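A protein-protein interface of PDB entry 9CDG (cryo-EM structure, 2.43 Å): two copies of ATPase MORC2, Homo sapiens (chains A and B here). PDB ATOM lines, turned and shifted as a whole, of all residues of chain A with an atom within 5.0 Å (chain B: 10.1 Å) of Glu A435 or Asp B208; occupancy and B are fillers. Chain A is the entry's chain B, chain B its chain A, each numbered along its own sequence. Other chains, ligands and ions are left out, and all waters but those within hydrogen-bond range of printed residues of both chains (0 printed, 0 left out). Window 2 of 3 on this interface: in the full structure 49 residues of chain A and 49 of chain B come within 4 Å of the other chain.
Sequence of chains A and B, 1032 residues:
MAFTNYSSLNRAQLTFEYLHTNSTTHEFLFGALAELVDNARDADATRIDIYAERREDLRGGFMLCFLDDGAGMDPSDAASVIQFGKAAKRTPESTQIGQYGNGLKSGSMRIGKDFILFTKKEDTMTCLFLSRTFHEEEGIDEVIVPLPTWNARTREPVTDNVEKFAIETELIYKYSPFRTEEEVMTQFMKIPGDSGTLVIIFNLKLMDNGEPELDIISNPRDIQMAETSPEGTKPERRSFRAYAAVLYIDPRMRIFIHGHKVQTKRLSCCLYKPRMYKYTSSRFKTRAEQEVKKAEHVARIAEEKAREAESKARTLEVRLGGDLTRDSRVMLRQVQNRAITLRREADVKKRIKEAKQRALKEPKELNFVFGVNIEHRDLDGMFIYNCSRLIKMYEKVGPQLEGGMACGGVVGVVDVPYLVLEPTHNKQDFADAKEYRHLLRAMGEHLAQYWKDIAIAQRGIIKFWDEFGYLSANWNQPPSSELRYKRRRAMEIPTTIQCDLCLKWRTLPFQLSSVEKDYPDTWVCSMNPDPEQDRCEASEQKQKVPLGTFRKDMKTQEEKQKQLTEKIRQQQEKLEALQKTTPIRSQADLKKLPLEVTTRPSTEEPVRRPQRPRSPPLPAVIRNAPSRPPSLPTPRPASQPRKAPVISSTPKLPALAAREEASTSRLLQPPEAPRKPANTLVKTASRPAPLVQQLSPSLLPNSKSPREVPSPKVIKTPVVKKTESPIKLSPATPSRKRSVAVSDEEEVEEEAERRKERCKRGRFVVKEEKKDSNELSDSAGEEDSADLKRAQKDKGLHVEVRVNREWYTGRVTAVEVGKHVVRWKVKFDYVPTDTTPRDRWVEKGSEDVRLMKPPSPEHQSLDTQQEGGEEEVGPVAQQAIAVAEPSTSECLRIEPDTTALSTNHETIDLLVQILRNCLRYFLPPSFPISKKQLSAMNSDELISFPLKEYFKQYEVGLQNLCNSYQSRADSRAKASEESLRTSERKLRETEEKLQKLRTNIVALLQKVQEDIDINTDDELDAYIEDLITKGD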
ATOM      1  N   ARG A 283     -33.094   3.130  18.198  1.00  0.00           N
ATOM      2  CA  ARG A 283     -33.042   2.209  17.065  1.00  0.00           C
ATOM      3  C   ARG A 283     -34.150   1.165  17.149  1.00  0.00           C
ATOM      4  O   ARG A 283     -34.671   0.718  16.120  1.00  0.00           O
ATOM      5  CB  ARG A 283     -31.659   1.549  17.020  1.00  0.00           C
ATOM      6  CG  ARG A 283     -31.279   0.739  15.768  1.00  0.00           C
ATOM      7  CD  ARG A 283     -31.876   1.231  14.458  1.00  0.00           C
ATOM      8  NE  ARG A 283     -31.836   0.170  13.457  1.00  0.00           N
ATOM      9  CZ  ARG A 283     -30.840  -0.030  12.604  1.00  0.00           C
ATOM     10  NH1 ARG A 283     -29.845   0.828  12.490  1.00  0.00           N
ATOM     11  NH2 ARG A 283     -30.850  -1.113  11.834  1.00  0.00           N
ATOM     12  N   THR A 286     -37.471   3.400  16.257  1.00  0.00           N
ATOM     13  CA  THR A 286     -37.562   4.015  14.935  1.00  0.00           C
ATOM     14  C   THR A 286     -37.908   2.991  13.860  1.00  0.00           C
ATOM     15  O   THR A 286     -38.796   3.226  13.032  1.00  0.00           O
ATOM     16  CB  THR A 286     -36.255   4.725  14.588  1.00  0.00           C
ATOM     17  OG1 THR A 286     -35.768   5.418  15.744  1.00  0.00           O
ATOM     18  CG2 THR A 286     -36.479   5.726  13.468  1.00  0.00           C
ATOM     19  N   GLN A 290     -40.840   2.254  11.522  1.00  0.00           N
ATOM     20  CA  GLN A 290     -40.606   2.200  10.084  1.00  0.00           C
ATOM     21  C   GLN A 290     -41.269   0.992   9.437  1.00  0.00           C
ATOM     22  O   GLN A 290     -41.705   1.079   8.285  1.00  0.00           O
ATOM     23  CB  GLN A 290     -39.107   2.188   9.784  1.00  0.00           C
ATOM     24  CG  GLN A 290     -38.511   3.564   9.560  1.00  0.00           C
ATOM     25  CD  GLN A 290     -37.004   3.574   9.707  1.00  0.00           C
ATOM     26  OE1 GLN A 290     -36.333   2.591   9.397  1.00  0.00           O
ATOM     27  NE2 GLN A 290     -36.464   4.689  10.182  1.00  0.00           N
ATOM     28  N   LEU A 421     -31.243  -4.973  14.838  1.00  0.00           N
ATOM     29  CA  LEU A 421     -30.022  -5.267  14.111  1.00  0.00           C
ATOM     30  C   LEU A 421     -30.227  -6.502  13.253  1.00  0.00           C
ATOM     31  O   LEU A 421     -30.920  -7.441  13.652  1.00  0.00           O
ATOM     32  CB  LEU A 421     -28.845  -5.483  15.065  1.00  0.00           C
ATOM     33  CG  LEU A 421     -28.105  -4.221  15.496  1.00  0.00           C
ATOM     34  CD1 LEU A 421     -27.193  -4.518  16.666  1.00  0.00           C
ATOM     35  CD2 LEU A 421     -27.319  -3.663  14.330  1.00  0.00           C
ATOM     36  N   ASP A 432     -25.476  -3.159  10.163  1.00  0.00           N
ATOM     37  CA  ASP A 432     -25.481  -1.747  10.542  1.00  0.00           C
ATOM     38  C   ASP A 432     -24.381  -1.530  11.569  1.00  0.00           C
ATOM     39  O   ASP A 432     -24.592  -1.645  12.778  1.00  0.00           O
ATOM     40  CB  ASP A 432     -26.844  -1.333  11.079  1.00  0.00           C
ATOM     41  CG  ASP A 432     -27.108   0.148  10.908  1.00  0.00           C
ATOM     42  OD1 ASP A 432     -26.277   0.960  11.363  1.00  0.00           O
ATOM     43  OD2 ASP A 432     -28.148   0.502  10.313  1.00  0.00           O
ATOM     44  N   ALA A 433     -23.187  -1.201  11.072  1.00  0.00           N
ATOM     45  CA  ALA A 433     -22.038  -0.980  11.939  1.00  0.00           C
ATOM     46  C   ALA A 433     -22.182   0.270  12.791  1.00  0.00           C
ATOM     47  O   ALA A 433     -21.682   0.286  13.920  1.00  0.00           O
ATOM     48  CB  ALA A 433     -20.763  -0.889  11.105  1.00  0.00           C
ATOM     49  N   LYS A 434     -22.871   1.297  12.286  1.00  0.00           N
ATOM     50  CA  LYS A 434     -23.045   2.534  13.042  1.00  0.00           C
ATOM     51  C   LYS A 434     -23.901   2.311  14.283  1.00  0.00           C
ATOM     52  O   LYS A 434     -23.506   2.675  15.398  1.00  0.00           O
ATOM     53  CB  LYS A 434     -23.666   3.605  12.145  1.00  0.00           C
ATOM     54  CG  LYS A 434     -24.282   4.769  12.899  1.00  0.00           C
ATOM     55  CD  LYS A 434     -24.822   5.814  11.949  1.00  0.00           C
ATOM     56  CE  LYS A 434     -25.416   6.986  12.705  1.00  0.00           C
ATOM     57  NZ  LYS A 434     -26.730   6.633  13.305  1.00  0.00           N
ATOM     58  N   GLU A 435     -25.063   1.684  14.121  1.00  0.00           N
ATOM     59  CA  GLU A 435     -25.882   1.409  15.290  1.00  0.00           C
ATOM     60  C   GLU A 435     -25.380   0.225  16.100  1.00  0.00           C
ATOM     61  O   GLU A 435     -25.716   0.131  17.283  1.00  0.00           O
ATOM     62  CB  GLU A 435     -27.339   1.205  14.885  1.00  0.00           C
ATOM     63  CG  GLU A 435     -28.068   2.524  14.682  1.00  0.00           C
ATOM     64  CD  GLU A 435     -28.287   3.278  15.976  1.00  0.00           C
ATOM     65  OE1 GLU A 435     -28.512   2.625  17.016  1.00  0.00           O
ATOM     66  OE2 GLU A 435     -28.237   4.525  15.952  1.00  0.00           O
ATOM     67  N   TYR A 436     -24.551  -0.647  15.521  1.00  0.00           N
ATOM     68  CA  TYR A 436     -23.842  -1.621  16.344  1.00  0.00           C
ATOM     69  C   TYR A 436     -22.849  -0.928  17.273  1.00  0.00           C
ATOM     70  O   TYR A 436     -22.733  -1.292  18.447  1.00  0.00           O
ATOM     71  CB  TYR A 436     -23.124  -2.644  15.465  1.00  0.00           C
ATOM     72  CG  TYR A 436     -22.252  -3.588  16.258  1.00  0.00           C
ATOM     73  CD1 TYR A 436     -20.929  -3.808  15.903  1.00  0.00           C
ATOM     74  CD2 TYR A 436     -22.765  -4.289  17.345  1.00  0.00           C
ATOM     75  CE1 TYR A 436     -20.131  -4.668  16.631  1.00  0.00           C
ATOM     76  CE2 TYR A 436     -21.981  -5.151  18.070  1.00  0.00           C
ATOM     77  CZ  TYR A 436     -20.667  -5.337  17.711  1.00  0.00           C
ATOM     78  OH  TYR A 436     -19.889  -6.198  18.444  1.00  0.00           O
ATOM     79  N   ARG A 437     -22.128   0.077  16.766  1.00  0.00           N
ATOM     80  CA  ARG A 437     -21.232   0.853  17.617  1.00  0.00           C
ATOM     81  C   ARG A 437     -22.002   1.680  18.636  1.00  0.00           C
ATOM     82  O   ARG A 437     -21.520   1.884  19.755  1.00  0.00           O
ATOM     83  CB  ARG A 437     -20.347   1.758  16.765  1.00  0.00           C
ATOM     84  CG  ARG A 437     -19.194   1.043  16.088  1.00  0.00           C
ATOM     85  CD  ARG A 437     -18.312   2.028  15.346  1.00  0.00           C
ATOM     86  NE  ARG A 437     -18.978   2.574  14.171  1.00  0.00           N
ATOM     87  CZ  ARG A 437     -18.966   2.005  12.975  1.00  0.00           C
ATOM     88  NH1 ARG A 437     -18.314   0.876  12.753  1.00  0.00           N
ATOM     89  NH2 ARG A 437     -19.619   2.587  11.974  1.00  0.00           N
ATOM     90  N   HIS A 438     -23.189   2.164  18.259  1.00  0.00           N
ATOM     91  CA  HIS A 438     -24.077   2.824  19.213  1.00  0.00           C
ATOM     92  C   HIS A 438     -24.493   1.872  20.329  1.00  0.00           C
ATOM     93  O   HIS A 438     -24.509   2.250  21.509  1.00  0.00           O
ATOM     94  CB  HIS A 438     -25.306   3.362  18.480  1.00  0.00           C
ATOM     95  CG  HIS A 438     -26.217   4.185  19.335  1.00  0.00           C
ATOM     96  ND1 HIS A 438     -27.533   4.418  19.003  1.00  0.00           N
ATOM     97  CD2 HIS A 438     -26.002   4.841  20.500  1.00  0.00           C
ATOM     98  CE1 HIS A 438     -28.093   5.174  19.929  1.00  0.00           C
ATOM     99  NE2 HIS A 438     -27.185   5.444  20.849  1.00  0.00           N
ATOM    100  N   LEU A 439     -24.818   0.629  19.966  1.00  0.00           N
ATOM    101  CA  LEU A 439     -25.154  -0.402  20.941  1.00  0.00           C
ATOM    102  C   LEU A 439     -23.982  -0.708  21.860  1.00  0.00           C
ATOM    103  O   LEU A 439     -24.163  -0.862  23.070  1.00  0.00           O
ATOM    104  CB  LEU A 439     -25.593  -1.669  20.215  1.00  0.00           C
ATOM    105  CG  LEU A 439     -26.303  -2.718  21.057  1.00  0.00           C
ATOM    106  CD1 LEU A 439     -27.779  -2.446  21.029  1.00  0.00           C
ATOM    107  CD2 LEU A 439     -25.999  -4.107  20.535  1.00  0.00           C
ATOM    108  N   GLU B  27     -20.236  -5.079   6.066  1.00  0.00           N
ATOM    109  CA  GLU B  27     -20.251  -4.209   7.232  1.00  0.00           C
ATOM    110  C   GLU B  27     -19.561  -2.888   6.923  1.00  0.00           C
ATOM    111  O   GLU B  27     -19.970  -1.836   7.427  1.00  0.00           O
ATOM    112  CB  GLU B  27     -19.587  -4.929   8.409  1.00  0.00           C
ATOM    113  CG  GLU B  27     -19.501  -4.140   9.701  1.00  0.00           C
ATOM    114  CD  GLU B  27     -18.132  -3.524   9.908  1.00  0.00           C
ATOM    115  OE1 GLU B  27     -17.167  -4.284  10.131  1.00  0.00           O
ATOM    116  OE2 GLU B  27     -18.017  -2.283   9.840  1.00  0.00           O
ATOM    117  N   ARG B 110     -25.319  -3.125  -1.334  1.00  0.00           N
ATOM    118  CA  ARG B 110     -25.073  -2.564  -0.012  1.00  0.00           C
ATOM    119  C   ARG B 110     -25.311  -1.057   0.000  1.00  0.00           C
ATOM    120  O   ARG B 110     -25.906  -0.529   0.945  1.00  0.00           O
ATOM    121  CB  ARG B 110     -23.656  -2.894   0.445  1.00  0.00           C
ATOM    122  CG  ARG B 110     -23.272  -2.245   1.753  1.00  0.00           C
ATOM    123  CD  ARG B 110     -24.122  -2.744   2.896  1.00  0.00           C
ATOM    124  NE  ARG B 110     -23.762  -2.089   4.145  1.00  0.00           N
ATOM    125  CZ  ARG B 110     -24.270  -0.936   4.556  1.00  0.00           C
ATOM    126  NH1 ARG B 110     -25.180  -0.291   3.846  1.00  0.00           N
ATOM    127  NH2 ARG B 110     -23.854  -0.417   5.707  1.00  0.00           N
ATOM    128  N   LYS B 205     -29.404   3.563   0.720  1.00  0.00           N
ATOM    129  CA  LYS B 205     -29.887   3.210   2.044  1.00  0.00           C
ATOM    130  C   LYS B 205     -29.854   4.422   2.961  1.00  0.00           C
ATOM    131  O   LYS B 205     -28.908   5.213   2.941  1.00  0.00           O
ATOM    132  CB  LYS B 205     -29.044   2.088   2.644  1.00  0.00           C
ATOM    133  CG  LYS B 205     -28.810   0.922   1.715  1.00  0.00           C
ATOM    134  CD  LYS B 205     -30.069   0.115   1.517  1.00  0.00           C
ATOM    135  CE  LYS B 205     -29.853  -0.964   0.484  1.00  0.00           C
ATOM    136  NZ  LYS B 205     -29.598  -2.288   1.110  1.00  0.00           N
ATOM    137  N   LEU B 206     -30.900   4.564   3.762  1.00  0.00           N
ATOM    138  CA  LEU B 206     -31.004   5.644   4.724  1.00  0.00           C
ATOM    139  C   LEU B 206     -30.613   5.143   6.105  1.00  0.00           C
ATOM    140  O   LEU B 206     -30.544   3.938   6.359  1.00  0.00           O
ATOM    141  CB  LEU B 206     -32.425   6.214   4.762  1.00  0.00           C
ATOM    142  CG  LEU B 206     -33.060   6.606   3.430  1.00  0.00           C
ATOM    143  CD1 LEU B 206     -34.405   7.259   3.665  1.00  0.00           C
ATOM    144  CD2 LEU B 206     -32.151   7.538   2.668  1.00  0.00           C
ATOM    145  N   MET B 207     -30.346   6.086   6.993  1.00  0.00           N
ATOM    146  CA  MET B 207     -30.121   5.773   8.393  1.00  0.00           C
ATOM    147  C   MET B 207     -31.450   5.863   9.137  1.00  0.00           C
ATOM    148  O   MET B 207     -32.525   5.880   8.530  1.00  0.00           O
ATOM    149  CB  MET B 207     -29.058   6.695   8.975  1.00  0.00           C
ATOM    150  CG  MET B 207     -27.721   6.572   8.286  1.00  0.00           C
ATOM    151  SD  MET B 207     -26.456   7.533   9.114  1.00  0.00           S
ATOM    152  CE  MET B 207     -27.229   9.145   9.144  1.00  0.00           C
ATOM    153  N   ASP B 208     -31.390   5.894  10.471  1.00  0.00           N
ATOM    154  CA  ASP B 208     -32.607   5.976  11.271  1.00  0.00           C
ATOM    155  C   ASP B 208     -33.299   7.325  11.119  1.00  0.00           C
ATOM    156  O   ASP B 208     -34.529   7.402  11.210  1.00  0.00           O
ATOM    157  CB  ASP B 208     -32.284   5.709  12.741  1.00  0.00           C
ATOM    158  CG  ASP B 208     -31.010   6.401  13.196  1.00  0.00           C
ATOM    159  OD1 ASP B 208     -30.432   7.175  12.403  1.00  0.00           O
ATOM    160  OD2 ASP B 208     -30.588   6.171  14.349  1.00  0.00           O
ATOM    161  N   ASN B 209     -32.538   8.389  10.876  1.00  0.00           N
ATOM    162  CA  ASN B 209     -33.094   9.727  10.748  1.00  0.00           C
ATOM    163  C   ASN B 209     -33.512  10.065   9.324  1.00  0.00           C
ATOM    164  O   ASN B 209     -33.946  11.193   9.075  1.00  0.00           O
ATOM    165  CB  ASN B 209     -32.085  10.766  11.244  1.00  0.00           C
ATOM    166  CG  ASN B 209     -30.696  10.527  10.701  1.00  0.00           C
ATOM    167  OD1 ASN B 209     -30.463   9.574   9.963  1.00  0.00           O
ATOM    168  ND2 ASN B 209     -29.761  11.392  11.070  1.00  0.00           N
ATOM    169  N   GLY B 210     -33.388   9.128   8.391  1.00  0.00           N
ATOM    170  CA  GLY B 210     -33.743   9.368   7.011  1.00  0.00           C
ATOM    171  C   GLY B 210     -32.631   9.932   6.158  1.00  0.00           C
ATOM    172  O   GLY B 210     -32.792  10.016   4.935  1.00  0.00           O
ATOM    173  N   GLU B 211     -31.516  10.326   6.760  1.00  0.00           N
ATOM    174  CA  GLU B 211     -30.378  10.784   5.989  1.00  0.00           C
ATOM    175  C   GLU B 211     -29.662   9.591   5.361  1.00  0.00           C
ATOM    176  O   GLU B 211     -29.680   8.489   5.915  1.00  0.00           O
ATOM    177  CB  GLU B 211     -29.416  11.565   6.881  1.00  0.00           C
ATOM    178  CG  GLU B 211     -29.899  12.962   7.231  1.00  0.00           C
ATOM    179  CD  GLU B 211     -30.614  13.641   6.078  1.00  0.00           C
ATOM    180  OE1 GLU B 211     -29.940  14.019   5.099  1.00  0.00           O
ATOM    181  OE2 GLU B 211     -31.852  13.799   6.154  1.00  0.00           O
ATOM    182  N   PRO B 212     -29.049   9.773   4.193  1.00  0.00           N
ATOM    183  CA  PRO B 212     -28.256   8.691   3.603  1.00  0.00           C
ATOM    184  C   PRO B 212     -27.001   8.419   4.415  1.00  0.00           C
ATOM    185  O   PRO B 212     -26.488   9.281   5.132  1.00  0.00           O
ATOM    186  CB  PRO B 212     -27.911   9.220   2.209  1.00  0.00           C
ATOM    187  CG  PRO B 212     -28.009  10.691   2.335  1.00  0.00           C
ATOM    188  CD  PRO B 212     -29.125  10.937   3.296  1.00  0.00           C
ATOM    189  N   GLU B 213     -26.516   7.180   4.302  1.00  0.00           N
ATOM    190  CA  GLU B 213     -25.353   6.761   5.072  1.00  0.00           C
ATOM    191  C   GLU B 213     -24.067   7.416   4.592  1.00  0.00           C
ATOM    192  O   GLU B 213     -23.126   7.554   5.381  1.00  0.00           O
ATOM    193  CB  GLU B 213     -25.200   5.244   5.014  1.00  0.00           C
ATOM    194  CG  GLU B 213     -26.498   4.483   5.155  1.00  0.00           C
ATOM    195  CD  GLU B 213     -26.298   2.986   5.072  1.00  0.00           C
ATOM    196  OE1 GLU B 213     -26.005   2.485   3.968  1.00  0.00           O
ATOM    197  OE2 GLU B 213     -26.433   2.308   6.111  1.00  0.00           O
ATOM    198  N   ALA B 226     -21.825   9.091   7.602  1.00  0.00           N
ATOM    199  CA  ALA B 226     -22.720  10.107   8.152  1.00  0.00           C
ATOM    200  C   ALA B 226     -22.930   9.831   9.639  1.00  0.00           C
ATOM    201  O   ALA B 226     -23.975   9.347  10.078  1.00  0.00           O
ATOM    202  CB  ALA B 226     -24.037  10.129   7.390  1.00  0.00           C
ATOM    203  N   GLU B 227     -21.916  10.164  10.433  1.00  0.00           N
ATOM    204  CA  GLU B 227     -21.974   9.923  11.866  1.00  0.00           C
ATOM    205  C   GLU B 227     -21.053  10.896  12.584  1.00  0.00           C
ATOM    206  O   GLU B 227     -20.173  11.514  11.979  1.00  0.00           O
ATOM    207  CB  GLU B 227     -21.583   8.483  12.216  1.00  0.00           C
ATOM    208  CG  GLU B 227     -20.463   7.910  11.362  1.00  0.00           C
ATOM    209  CD  GLU B 227     -19.082   8.352  11.811  1.00  0.00           C
ATOM    210  OE1 GLU B 227     -18.823   8.341  13.032  1.00  0.00           O
ATOM    211  OE2 GLU B 227     -18.261   8.719  10.946  1.00  0.00           O
ATOM    212  N   THR B 228     -21.264  11.015  13.893  1.00  0.00           N
ATOM    213  CA  THR B 228     -20.336  11.736  14.752  1.00  0.00           C
ATOM    214  C   THR B 228     -19.129  10.848  15.014  1.00  0.00           C
ATOM    215  O   THR B 228     -19.260   9.772  15.608  1.00  0.00           O
ATOM    216  CB  THR B 228     -21.008  12.130  16.065  1.00  0.00           C
ATOM    217  OG1 THR B 228     -21.360  10.950  16.796  1.00  0.00           O
ATOM    218  CG2 THR B 228     -22.263  12.945  15.796  1.00  0.00           C
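OD1 of Asp A432 lies within hydrogen-bond range of N of Glu A435, 3.1 Å away. The side-chain amino group (NZ) of Lys A434 is in salt-bridge range of the side-chain carboxylate (OE2) of Glu A435. The side-chain carboxylate (OE1) of Glu A435 lies within hydrogen-bond range of a ring nitrogen (ND1) of His A438. The side-chain carboxylate (OD1) of Asp B208 sits close to the side-chain amide oxygen (OD1) of Asn B209. The backbone carbonyl oxygen (O) of Glu B213 lies within hydrogen-bond range of the backbone NH (N) of Ala B226, 3.0 Å away.
Of the printed residues of chain B, Gln A290 touches Asp B208. Of chain B, only Glu B27 (3.3 Å) comes within 4 Å of Ala A433. Of chain B, only Met B207 (3.7 Å), Asp B208 (3.8 Å) and Ala B226 (3.8 Å) come within 4 Å of Lys A434. Of chain B, only Asp B208 (3.3 Å) comes within 4 Å of Glu A435. No residue of chain B comes within 4 Å of His A438. Printed residues of chain A within 4 Å of Glu B27: Ala A433. Of chain A, only Thr A286 (3.4 Å), Gln A290 (3.5 Å), Lys A434 (3.8 Å) and Glu A435 (3.3 Å) come within 4 Å of Asp B208. Of the printed residues of chain A, Ala B226 touches Lys A434. The nearest residue of chain B that does not touch Glu A435 is Met B207 (7.1 Å). The nearest printed residue of chain A that does not touch Met B207 is Gln A290 (4.4 Å).
Among the printed residues, pairs that only touch across the chains: Thr A286 with Asp B208, Ala A433 with Glu B27, Lys A434 with Met B207 and Lys A434 with Ala B226.
Hydrophobic or aromatic side chains of chain B that line the printed part of chain A: Met B207. Of the 12 printed residues of chain A, 5 touch a printed residue of chain B. Hydrophobic or aromatic side chains of chain A that line the printed part of chain B: Ala A433. Among the printed residues, Asp or Glu carboxylates within 4 Å of a Lys or Arg side-chain nitrogen of the other chain: Lys A434 with Asp B208 (3.8 Å).
NE2 of Gln A290 is in hydrogen-bond range of O of Asp B208, 3.5 Å away. OD1 of Asp B208 is in salt-bridge range of NZ of Lys A434, at 3.8 Å. OE2 of Glu A435 sits close to OD2 of Asp B208.
No position is printed for both chains.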
